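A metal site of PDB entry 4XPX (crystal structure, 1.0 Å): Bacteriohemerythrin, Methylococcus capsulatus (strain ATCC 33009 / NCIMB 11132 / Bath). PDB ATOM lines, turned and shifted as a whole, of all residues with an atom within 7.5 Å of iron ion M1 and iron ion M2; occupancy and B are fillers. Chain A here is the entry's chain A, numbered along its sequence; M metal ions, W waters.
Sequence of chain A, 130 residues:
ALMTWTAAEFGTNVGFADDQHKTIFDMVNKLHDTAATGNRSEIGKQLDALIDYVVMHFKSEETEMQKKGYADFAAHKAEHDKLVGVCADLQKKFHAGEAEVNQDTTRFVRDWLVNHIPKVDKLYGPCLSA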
ATOM      1  N   THR A  12      -1.258 -33.016 -14.620  1.00  0.00           N
ATOM      2  CA  THR A  12      -1.494 -33.955 -13.544  1.00  0.00           C
ATOM      3  C   THR A  12      -2.094 -35.236 -13.992  1.00  0.00           C
ATOM      4  O   THR A  12      -2.192 -36.180 -13.173  1.00  0.00           O
ATOM      5  CB  THR A  12      -2.402 -33.373 -12.466  1.00  0.00           C
ATOM      6  OG1 THR A  12      -3.709 -33.177 -13.011  1.00  0.00           O
ATOM      7  CG2 THR A  12      -1.837 -32.108 -11.836  1.00  0.00           C
ATOM      8  N   ALA A  17      -8.489 -30.953 -12.430  1.00  0.00           N
ATOM      9  CA  ALA A  17      -7.437 -30.235 -11.797  1.00  0.00           C
ATOM     10  C   ALA A  17      -6.665 -29.429 -12.769  1.00  0.00           C
ATOM     11  O   ALA A  17      -6.323 -28.250 -12.528  1.00  0.00           O
ATOM     12  CB  ALA A  17      -6.512 -31.197 -11.064  1.00  0.00           C
ATOM     13  N   ASP A  18      -6.336 -29.989 -13.916  1.00  0.00           N
ATOM     14  CA  ASP A  18      -5.670 -29.231 -14.954  1.00  0.00           C
ATOM     15  C   ASP A  18      -6.492 -28.011 -15.360  1.00  0.00           C
ATOM     16  O   ASP A  18      -5.940 -26.916 -15.554  1.00  0.00           O
ATOM     17  CB  ASP A  18      -5.401 -30.078 -16.177  1.00  0.00           C
ATOM     18  CG  ASP A  18      -4.342 -31.172 -15.935  1.00  0.00           C
ATOM     19  OD1 ASP A  18      -3.542 -31.138 -15.037  1.00  0.00           O
ATOM     20  OD2 ASP A  18      -4.368 -32.086 -16.850  1.00  0.00           O
ATOM     21  N   GLN A  20      -8.785 -26.365 -13.584  1.00  0.00           N
ATOM     22  CA  GLN A  20      -8.771 -25.359 -12.510  1.00  0.00           C
ATOM     23  C   GLN A  20      -7.425 -24.684 -12.428  1.00  0.00           C
ATOM     24  O   GLN A  20      -7.357 -23.458 -12.189  1.00  0.00           O
ATOM     25  CB  GLN A  20      -9.167 -26.021 -11.138  1.00  0.00           C
ATOM     26  CG  GLN A  20     -10.619 -26.466 -11.136  1.00  0.00           C
ATOM     27  CD  GLN A  20     -11.020 -27.115  -9.832  1.00  0.00           C
ATOM     28  OE1 GLN A  20     -10.252 -27.652  -9.094  1.00  0.00           O
ATOM     29  NE2 GLN A  20     -12.292 -26.945  -9.485  1.00  0.00           N
ATOM     30  N   HIS A  21      -6.336 -25.432 -12.637  1.00  0.00           N
ATOM     31  CA  HIS A  21      -5.003 -24.771 -12.657  1.00  0.00           C
ATOM     32  C   HIS A  21      -4.917 -23.746 -13.749  1.00  0.00           C
ATOM     33  O   HIS A  21      -4.374 -22.645 -13.570  1.00  0.00           O
ATOM     34  CB  HIS A  21      -3.903 -25.811 -12.814  1.00  0.00           C
ATOM     35  CG  HIS A  21      -3.770 -26.695 -11.612  1.00  0.00           C
ATOM     36  ND1 HIS A  21      -3.214 -27.962 -11.666  1.00  0.00           N
ATOM     37  CD2 HIS A  21      -4.106 -26.503 -10.296  1.00  0.00           C
ATOM     38  CE1 HIS A  21      -3.197 -28.454 -10.421  1.00  0.00           C
ATOM     39  NE2 HIS A  21      -3.749 -27.620  -9.551  1.00  0.00           N
ATOM     40  N   ILE A  24      -6.645 -20.671 -12.607  1.00  0.00           N
ATOM     41  CA  ILE A  24      -5.822 -19.967 -11.649  1.00  0.00           C
ATOM     42  C   ILE A  24      -4.751 -19.154 -12.364  1.00  0.00           C
ATOM     43  O   ILE A  24      -4.502 -17.986 -12.018  1.00  0.00           O
ATOM     44  CB  ILE A  24      -5.259 -20.931 -10.614  1.00  0.00           C
ATOM     45  CG1 ILE A  24      -6.344 -21.478  -9.709  1.00  0.00           C
ATOM     46  CG2 ILE A  24      -4.177 -20.264  -9.798  1.00  0.00           C
ATOM     47  CD1 ILE A  24      -5.968 -22.681  -8.881  1.00  0.00           C
ATOM     48  N   VAL A  54      -9.081 -20.067  -5.834  1.00  0.00           N
ATOM     49  CA  VAL A  54      -8.056 -20.935  -5.308  1.00  0.00           C
ATOM     50  C   VAL A  54      -8.623 -21.791  -4.159  1.00  0.00           C
ATOM     51  O   VAL A  54      -8.391 -23.033  -4.099  1.00  0.00           O
ATOM     52  CB  VAL A  54      -6.839 -20.166  -4.877  1.00  0.00           C
ATOM     53  CG1 VAL A  54      -5.845 -21.044  -4.086  1.00  0.00           C
ATOM     54  CG2 VAL A  54      -6.129 -19.595  -6.116  1.00  0.00           C
ATOM     55  N   HIS A  57     -10.701 -24.490  -5.596  1.00  0.00           N
ATOM     56  CA  HIS A  57      -9.859 -25.485  -6.209  1.00  0.00           C
ATOM     57  C   HIS A  57      -9.303 -26.437  -5.130  1.00  0.00           C
ATOM     58  O   HIS A  57      -9.284 -27.695  -5.311  1.00  0.00           O
ATOM     59  CB  HIS A  57      -8.725 -24.798  -6.951  1.00  0.00           C
ATOM     60  CG  HIS A  57      -7.624 -25.750  -7.362  1.00  0.00           C
ATOM     61  ND1 HIS A  57      -7.833 -26.845  -8.162  1.00  0.00           N
ATOM     62  CD2 HIS A  57      -6.320 -25.803  -7.008  1.00  0.00           C
ATOM     63  CE1 HIS A  57      -6.672 -27.514  -8.280  1.00  0.00           C
ATOM     64  NE2 HIS A  57      -5.733 -26.912  -7.577  1.00  0.00           N
ATOM     65  N   PHE A  58      -8.795 -25.888  -4.049  1.00  0.00           N
ATOM     66  CA  PHE A  58      -8.265 -26.726  -2.978  1.00  0.00           C
ATOM     67  C   PHE A  58      -9.322 -27.639  -2.458  1.00  0.00           C
ATOM     68  O   PHE A  58      -9.047 -28.848  -2.201  1.00  0.00           O
ATOM     69  CB  PHE A  58      -7.693 -25.859  -1.850  1.00  0.00           C
ATOM     70  CG  PHE A  58      -6.414 -25.097  -2.230  1.00  0.00           C
ATOM     71  CD1 PHE A  58      -5.974 -24.127  -1.327  1.00  0.00           C
ATOM     72  CD2 PHE A  58      -5.672 -25.367  -3.352  1.00  0.00           C
ATOM     73  CE1 PHE A  58      -4.799 -23.438  -1.572  1.00  0.00           C
ATOM     74  CE2 PHE A  58      -4.513 -24.648  -3.543  1.00  0.00           C
ATOM     75  CZ  PHE A  58      -4.058 -23.719  -2.673  1.00  0.00           C
ATOM     76  N   GLU A  61      -9.809 -30.556  -4.955  1.00  0.00           N
ATOM     77  CA  GLU A  61      -8.766 -31.560  -4.854  1.00  0.00           C
ATOM     78  C   GLU A  61      -8.948 -32.343  -3.536  1.00  0.00           C
ATOM     79  O   GLU A  61      -8.788 -33.607  -3.545  1.00  0.00           O
ATOM     80  CB  GLU A  61      -7.368 -30.932  -4.801  1.00  0.00           C
ATOM     81  CG  GLU A  61      -6.878 -30.383  -6.142  1.00  0.00           C
ATOM     82  CD  GLU A  61      -5.424 -29.941  -6.056  1.00  0.00           C
ATOM     83  OE1 GLU A  61      -4.883 -29.915  -4.971  1.00  0.00           O
ATOM     84  OE2 GLU A  61      -4.877 -29.631  -7.172  1.00  0.00           O
ATOM     85  N   GLU A  62      -9.212 -31.691  -2.454  1.00  0.00           N
ATOM     86  CA  GLU A  62      -9.277 -32.377  -1.150  1.00  0.00           C
ATOM     87  C   GLU A  62     -10.422 -33.337  -1.121  1.00  0.00           C
ATOM     88  O   GLU A  62     -10.269 -34.463  -0.558  1.00  0.00           O
ATOM     89  CB  GLU A  62      -9.398 -31.346  -0.027  1.00  0.00           C
ATOM     90  CG  GLU A  62      -8.113 -30.587   0.180  1.00  0.00           C
ATOM     91  CD  GLU A  62      -8.257 -29.297   0.951  1.00  0.00           C
ATOM     92  OE1 GLU A  62      -9.261 -29.162   1.755  1.00  0.00           O
ATOM     93  OE2 GLU A  62      -7.371 -28.399   0.887  1.00  0.00           O
ATOM     94  N   MET A  65      -9.311 -36.390  -3.210  1.00  0.00           N
ATOM     95  CA  MET A  65      -8.288 -37.127  -2.513  1.00  0.00           C
ATOM     96  C   MET A  65      -8.848 -37.904  -1.339  1.00  0.00           C
ATOM     97  O   MET A  65      -8.508 -39.119  -1.140  1.00  0.00           O
ATOM     98  CB  MET A  65      -7.174 -36.210  -2.001  1.00  0.00           C
ATOM     99  CG  MET A  65      -6.231 -35.711  -3.099  1.00  0.00           C
ATOM    100  SD  MET A  65      -4.814 -34.758  -2.431  1.00  0.00           S
ATOM    101  CE  MET A  65      -5.597 -33.158  -2.013  1.00  0.00           C
ATOM    102  N   HIS A  76      -0.992 -33.069   1.980  1.00  0.00           N
ATOM    103  CA  HIS A  76      -1.330 -32.176   0.882  1.00  0.00           C
ATOM    104  C   HIS A  76      -2.276 -31.114   1.343  1.00  0.00           C
ATOM    105  O   HIS A  76      -2.073 -29.881   1.075  1.00  0.00           O
ATOM    106  CB  HIS A  76      -1.912 -33.025  -0.237  1.00  0.00           C
ATOM    107  CG  HIS A  76      -2.098 -32.306  -1.517  1.00  0.00           C
ATOM    108  ND1 HIS A  76      -1.900 -32.972  -2.697  1.00  0.00           N
ATOM    109  CD2 HIS A  76      -2.525 -31.051  -1.850  1.00  0.00           C
ATOM    110  CE1 HIS A  76      -2.168 -32.081  -3.683  1.00  0.00           C
ATOM    111  NE2 HIS A  76      -2.568 -30.933  -3.220  1.00  0.00           N
ATOM    112  N   LYS A  77      -3.319 -31.466   2.086  1.00  0.00           N
ATOM    113  CA  LYS A  77      -4.229 -30.459   2.653  1.00  0.00           C
ATOM    114  C   LYS A  77      -3.495 -29.492   3.518  1.00  0.00           C
ATOM    115  O   LYS A  77      -3.835 -28.282   3.535  1.00  0.00           O
ATOM    116  CB  LYS A  77      -5.339 -31.142   3.412  1.00  0.00           C
ATOM    117  CG  LYS A  77      -6.329 -30.150   4.011  1.00  0.00           C
ATOM    118  CD  LYS A  77      -7.528 -30.816   4.590  1.00  0.00           C
ATOM    119  CE  LYS A  77      -8.610 -29.837   5.041  1.00  0.00           C
ATOM    120  NZ  LYS A  77      -8.144 -28.979   6.092  1.00  0.00           N
ATOM    121  N   GLU A  79      -0.502 -28.332   3.157  1.00  0.00           N
ATOM    122  CA  GLU A  79       0.112 -27.334   2.265  1.00  0.00           C
ATOM    123  C   GLU A  79      -0.900 -26.310   1.807  1.00  0.00           C
ATOM    124  O   GLU A  79      -0.657 -25.097   1.809  1.00  0.00           O
ATOM    125  CB  GLU A  79       0.799 -27.966   1.075  1.00  0.00           C
ATOM    126  CG  GLU A  79       1.854 -29.015   1.385  1.00  0.00           C
ATOM    127  CD  GLU A  79       3.005 -28.619   2.271  1.00  0.00           C
ATOM    128  OE1 GLU A  79       3.265 -27.410   2.429  1.00  0.00           O
ATOM    129  OE2 GLU A  79       3.688 -29.562   2.889  1.00  0.00           O
ATOM    130  N   HIS A  80      -2.056 -26.783   1.378  1.00  0.00           N
ATOM    131  CA  HIS A  80      -3.164 -25.860   0.979  1.00  0.00           C
ATOM    132  C   HIS A  80      -3.500 -24.938   2.103  1.00  0.00           C
ATOM    133  O   HIS A  80      -3.644 -23.693   1.896  1.00  0.00           O
ATOM    134  CB  HIS A  80      -4.411 -26.639   0.630  1.00  0.00           C
ATOM    135  CG  HIS A  80      -4.325 -27.445  -0.620  1.00  0.00           C
ATOM    136  ND1 HIS A  80      -5.353 -28.287  -0.971  1.00  0.00           N
ATOM    137  CD2 HIS A  80      -3.440 -27.520  -1.641  1.00  0.00           C
ATOM    138  CE1 HIS A  80      -5.048 -28.838  -2.156  1.00  0.00           C
ATOM    139  NE2 HIS A  80      -3.891 -28.355  -2.595  1.00  0.00           N
ATOM    140  N   TRP A 112       4.595 -20.229  -5.489  1.00  0.00           N
ATOM    141  CA  TRP A 112       3.930 -21.289  -4.741  1.00  0.00           C
ATOM    142  C   TRP A 112       3.342 -22.295  -5.722  1.00  0.00           C
ATOM    143  O   TRP A 112       3.501 -23.543  -5.517  1.00  0.00           O
ATOM    144  CB  TRP A 112       2.847 -20.685  -3.841  1.00  0.00           C
ATOM    145  CG  TRP A 112       2.240 -21.675  -2.907  1.00  0.00           C
ATOM    146  CD1 TRP A 112       2.638 -21.901  -1.605  1.00  0.00           C
ATOM    147  CD2 TRP A 112       1.212 -22.614  -3.182  1.00  0.00           C
ATOM    148  NE1 TRP A 112       1.903 -22.880  -1.060  1.00  0.00           N
ATOM    149  CE2 TRP A 112       1.010 -23.361  -2.003  1.00  0.00           C
ATOM    150  CE3 TRP A 112       0.406 -22.879  -4.250  1.00  0.00           C
ATOM    151  CZ2 TRP A 112       0.074 -24.373  -1.892  1.00  0.00           C
ATOM    152  CZ3 TRP A 112      -0.537 -23.869  -4.187  1.00  0.00           C
ATOM    153  CH2 TRP A 112      -0.687 -24.621  -2.978  1.00  0.00           C
ATOM    154  N   LEU A 113       2.669 -21.835  -6.763  1.00  0.00           N
ATOM    155  CA  LEU A 113       1.995 -22.722  -7.717  1.00  0.00           C
ATOM    156  C   LEU A 113       3.012 -23.540  -8.505  1.00  0.00           C
ATOM    157  O   LEU A 113       2.751 -24.759  -8.729  1.00  0.00           O
ATOM    158  CB  LEU A 113       1.163 -21.909  -8.696  1.00  0.00           C
ATOM    159  CG  LEU A 113      -0.110 -21.239  -8.071  1.00  0.00           C
ATOM    160  CD1 LEU A 113      -0.617 -20.160  -9.035  1.00  0.00           C
ATOM    161  CD2 LEU A 113      -1.179 -22.315  -7.838  1.00  0.00           C
ATOM    162  N   HIS A 116       4.148 -26.182  -6.118  1.00  0.00           N
ATOM    163  CA  HIS A 116       3.150 -27.111  -5.611  1.00  0.00           C
ATOM    164  C   HIS A 116       2.607 -28.031  -6.698  1.00  0.00           C
ATOM    165  O   HIS A 116       2.383 -29.221  -6.444  1.00  0.00           O
ATOM    166  CB  HIS A 116       1.939 -26.284  -5.079  1.00  0.00           C
ATOM    167  CG  HIS A 116       0.852 -27.120  -4.462  1.00  0.00           C
ATOM    168  ND1 HIS A 116       0.897 -27.578  -3.159  1.00  0.00           N
ATOM    169  CD2 HIS A 116      -0.296 -27.570  -4.999  1.00  0.00           C
ATOM    170  CE1 HIS A 116      -0.233 -28.250  -2.932  1.00  0.00           C
ATOM    171  NE2 HIS A 116      -0.999 -28.276  -4.008  1.00  0.00           N
ATOM    172  N   ILE A 117       2.327 -27.508  -7.884  1.00  0.00           N
ATOM    173  CA  ILE A 117       1.683 -28.341  -8.877  1.00  0.00           C
ATOM    174  C   ILE A 117       2.570 -29.531  -9.275  1.00  0.00           C
ATOM    175  O   ILE A 117       2.135 -30.671  -9.245  1.00  0.00           O
ATOM    176  CB  ILE A 117       1.127 -27.535 -10.046  1.00  0.00           C
ATOM    177  CG1 ILE A 117       0.011 -26.625  -9.565  1.00  0.00           C
ATOM    178  CG2 ILE A 117       0.653 -28.498 -11.151  1.00  0.00           C
ATOM    179  CD1 ILE A 117      -0.359 -25.538 -10.555  1.00  0.00           C
ATOM    180  N   VAL A 120       3.588 -31.636  -5.691  1.00  0.00           N
ATOM    181  CA  VAL A 120       2.555 -32.067  -4.762  1.00  0.00           C
ATOM    182  C   VAL A 120       1.347 -32.557  -5.562  1.00  0.00           C
ATOM    183  O   VAL A 120       0.920 -33.700  -5.397  1.00  0.00           O
ATOM    184  CB  VAL A 120       2.160 -30.939  -3.745  1.00  0.00           C
ATOM    185  CG1 VAL A 120       1.211 -31.505  -2.694  1.00  0.00           C
ATOM    186  CG2 VAL A 120       3.408 -30.361  -3.097  1.00  0.00           C
ATOM    187  N   ASP A 121       0.777 -31.750  -6.459  1.00  0.00           N
ATOM    188  CA  ASP A 121      -0.382 -32.185  -7.199  1.00  0.00           C
ATOM    189  C   ASP A 121      -0.092 -33.332  -8.131  1.00  0.00           C
ATOM    190  O   ASP A 121      -0.925 -34.258  -8.263  1.00  0.00           O
ATOM    191  CB  ASP A 121      -1.036 -31.032  -7.999  1.00  0.00           C
ATOM    192  CG  ASP A 121      -1.751 -30.010  -7.149  1.00  0.00           C
ATOM    193  OD1 ASP A 121      -2.003 -30.278  -5.957  1.00  0.00           O
ATOM    194  OD2 ASP A 121      -2.040 -28.927  -7.734  1.00  0.00           O
ATOM    195  N   LYS A 122       1.017 -33.341  -8.849  1.00  0.00           N
ATOM    196  CA  LYS A 122       1.242 -34.426  -9.771  1.00  0.00           C
ATOM    197  C   LYS A 122       1.175 -35.750  -9.070  1.00  0.00           C
ATOM    198  O   LYS A 122       0.880 -36.820  -9.712  1.00  0.00           O
ATOM    199  CB  LYS A 122       2.564 -34.281 -10.535  1.00  0.00           C
ATOM    200  CG  LYS A 122       2.491 -33.294 -11.670  1.00  0.00           C
ATOM    201  CD  LYS A 122       3.863 -33.306 -12.436  1.00  0.00           C
ATOM    202  CE  LYS A 122       3.874 -32.238 -13.515  1.00  0.00           C
ATOM    203  NZ  LYS A 122       5.022 -32.548 -14.437  1.00  0.00           N
ATOM    204  N   TYR A 124      -0.886 -36.983  -7.045  1.00  0.00           N
ATOM    205  CA  TYR A 124      -2.177 -37.621  -6.966  1.00  0.00           C
ATOM    206  C   TYR A 124      -2.684 -38.184  -8.279  1.00  0.00           C
ATOM    207  O   TYR A 124      -3.753 -38.745  -8.330  1.00  0.00           O
ATOM    208  CB  TYR A 124      -3.283 -36.722  -6.299  1.00  0.00           C
ATOM    209  CG  TYR A 124      -3.581 -35.404  -6.982  1.00  0.00           C
ATOM    210  CD1 TYR A 124      -3.852 -35.304  -8.333  1.00  0.00           C
ATOM    211  CD2 TYR A 124      -3.664 -34.230  -6.219  1.00  0.00           C
ATOM    212  CE1 TYR A 124      -4.154 -34.080  -8.933  1.00  0.00           C
ATOM    213  CE2 TYR A 124      -3.917 -33.026  -6.796  1.00  0.00           C
ATOM    214  CZ  TYR A 124      -4.149 -32.916  -8.136  1.00  0.00           C
ATOM    215  OH  TYR A 124      -4.380 -31.734  -8.796  1.00  0.00           O
HETATM  216 FE    FE M   1      -2.940 -29.130  -4.410  1.00  0.00          FE
HETATM  217 FE    FE M   2      -3.757 -27.732  -7.460  1.00  0.00          FE
HETATM  218  O   HOH W   1      -3.405 -27.232  -5.578  1.00  0.00           O
HETATM  219  O   HOH W   2      -2.655 -25.468  -7.358  1.00  0.00           O
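A ring nitrogen (ND1) of His 21 sits close to the backbone carbonyl oxygen (O) of Ala 17 (3.2 Å). ND1 of His 57 lies within hydrogen-bond range of OE1 of Gln 20 (2.7 Å). The side-chain carboxylate of Glu 61 lies close to the side-chain hydroxyl of Tyr 124. The side-chain carboxylate (OE2) of Glu 62 sits at hydrogen-bond distance from a ring nitrogen (ND1) of His 80 (2.7 Å). ND1 of His 76 is in hydrogen-bond range of SD of Met 65 (3.4 Å).
Within 4 Å of iron ion M1: Glu 61, His 76, His 80, His 116 and Asp 121. The nearest printed residue that does not touch iron ion M1 is Tyr 124 (4.7 Å).
Within 4 Å of iron ion M2: His 21, His 57, Glu 61 and Asp 121. Along chain A the residues within 4 Å of iron ion M2 span positions 21 to 121. The nearest printed residue that does not touch iron ion M2 is His 116 (4.2 Å).
OD1 of Asp 121 binds iron ion M1. A ring nitrogen (NE2) of His 116 binds iron ion M1. Iron ion M1 is bound by the side-chain carboxylate (OE1) of Glu 61, at 2.2 Å. Iron ion M1 is bound by a ring nitrogen (NE2) of His 80 (2.2 Å). NE2 of His 76 is bound to iron ion M1, at 2.2 Å. Water W1 is bound to iron ion M1.
Water W1 is bound to iron ion M2 (2.0 Å). NE2 of His 21 binds iron ion M2 (2.1 Å). Iron ion M2 is bound by OD2 of Asp 121 (2.1 Å). Iron ion M2 is bound by a ring nitrogen (NE2) of His 57, 2.1 Å away. The side-chain carboxylate (OE2) of Glu 61 binds iron ion M2, at 2.2 Å. Water W2 is bound to iron ion M2 (2.5 Å). Iron ion M2 has six donor atoms within binding distance.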
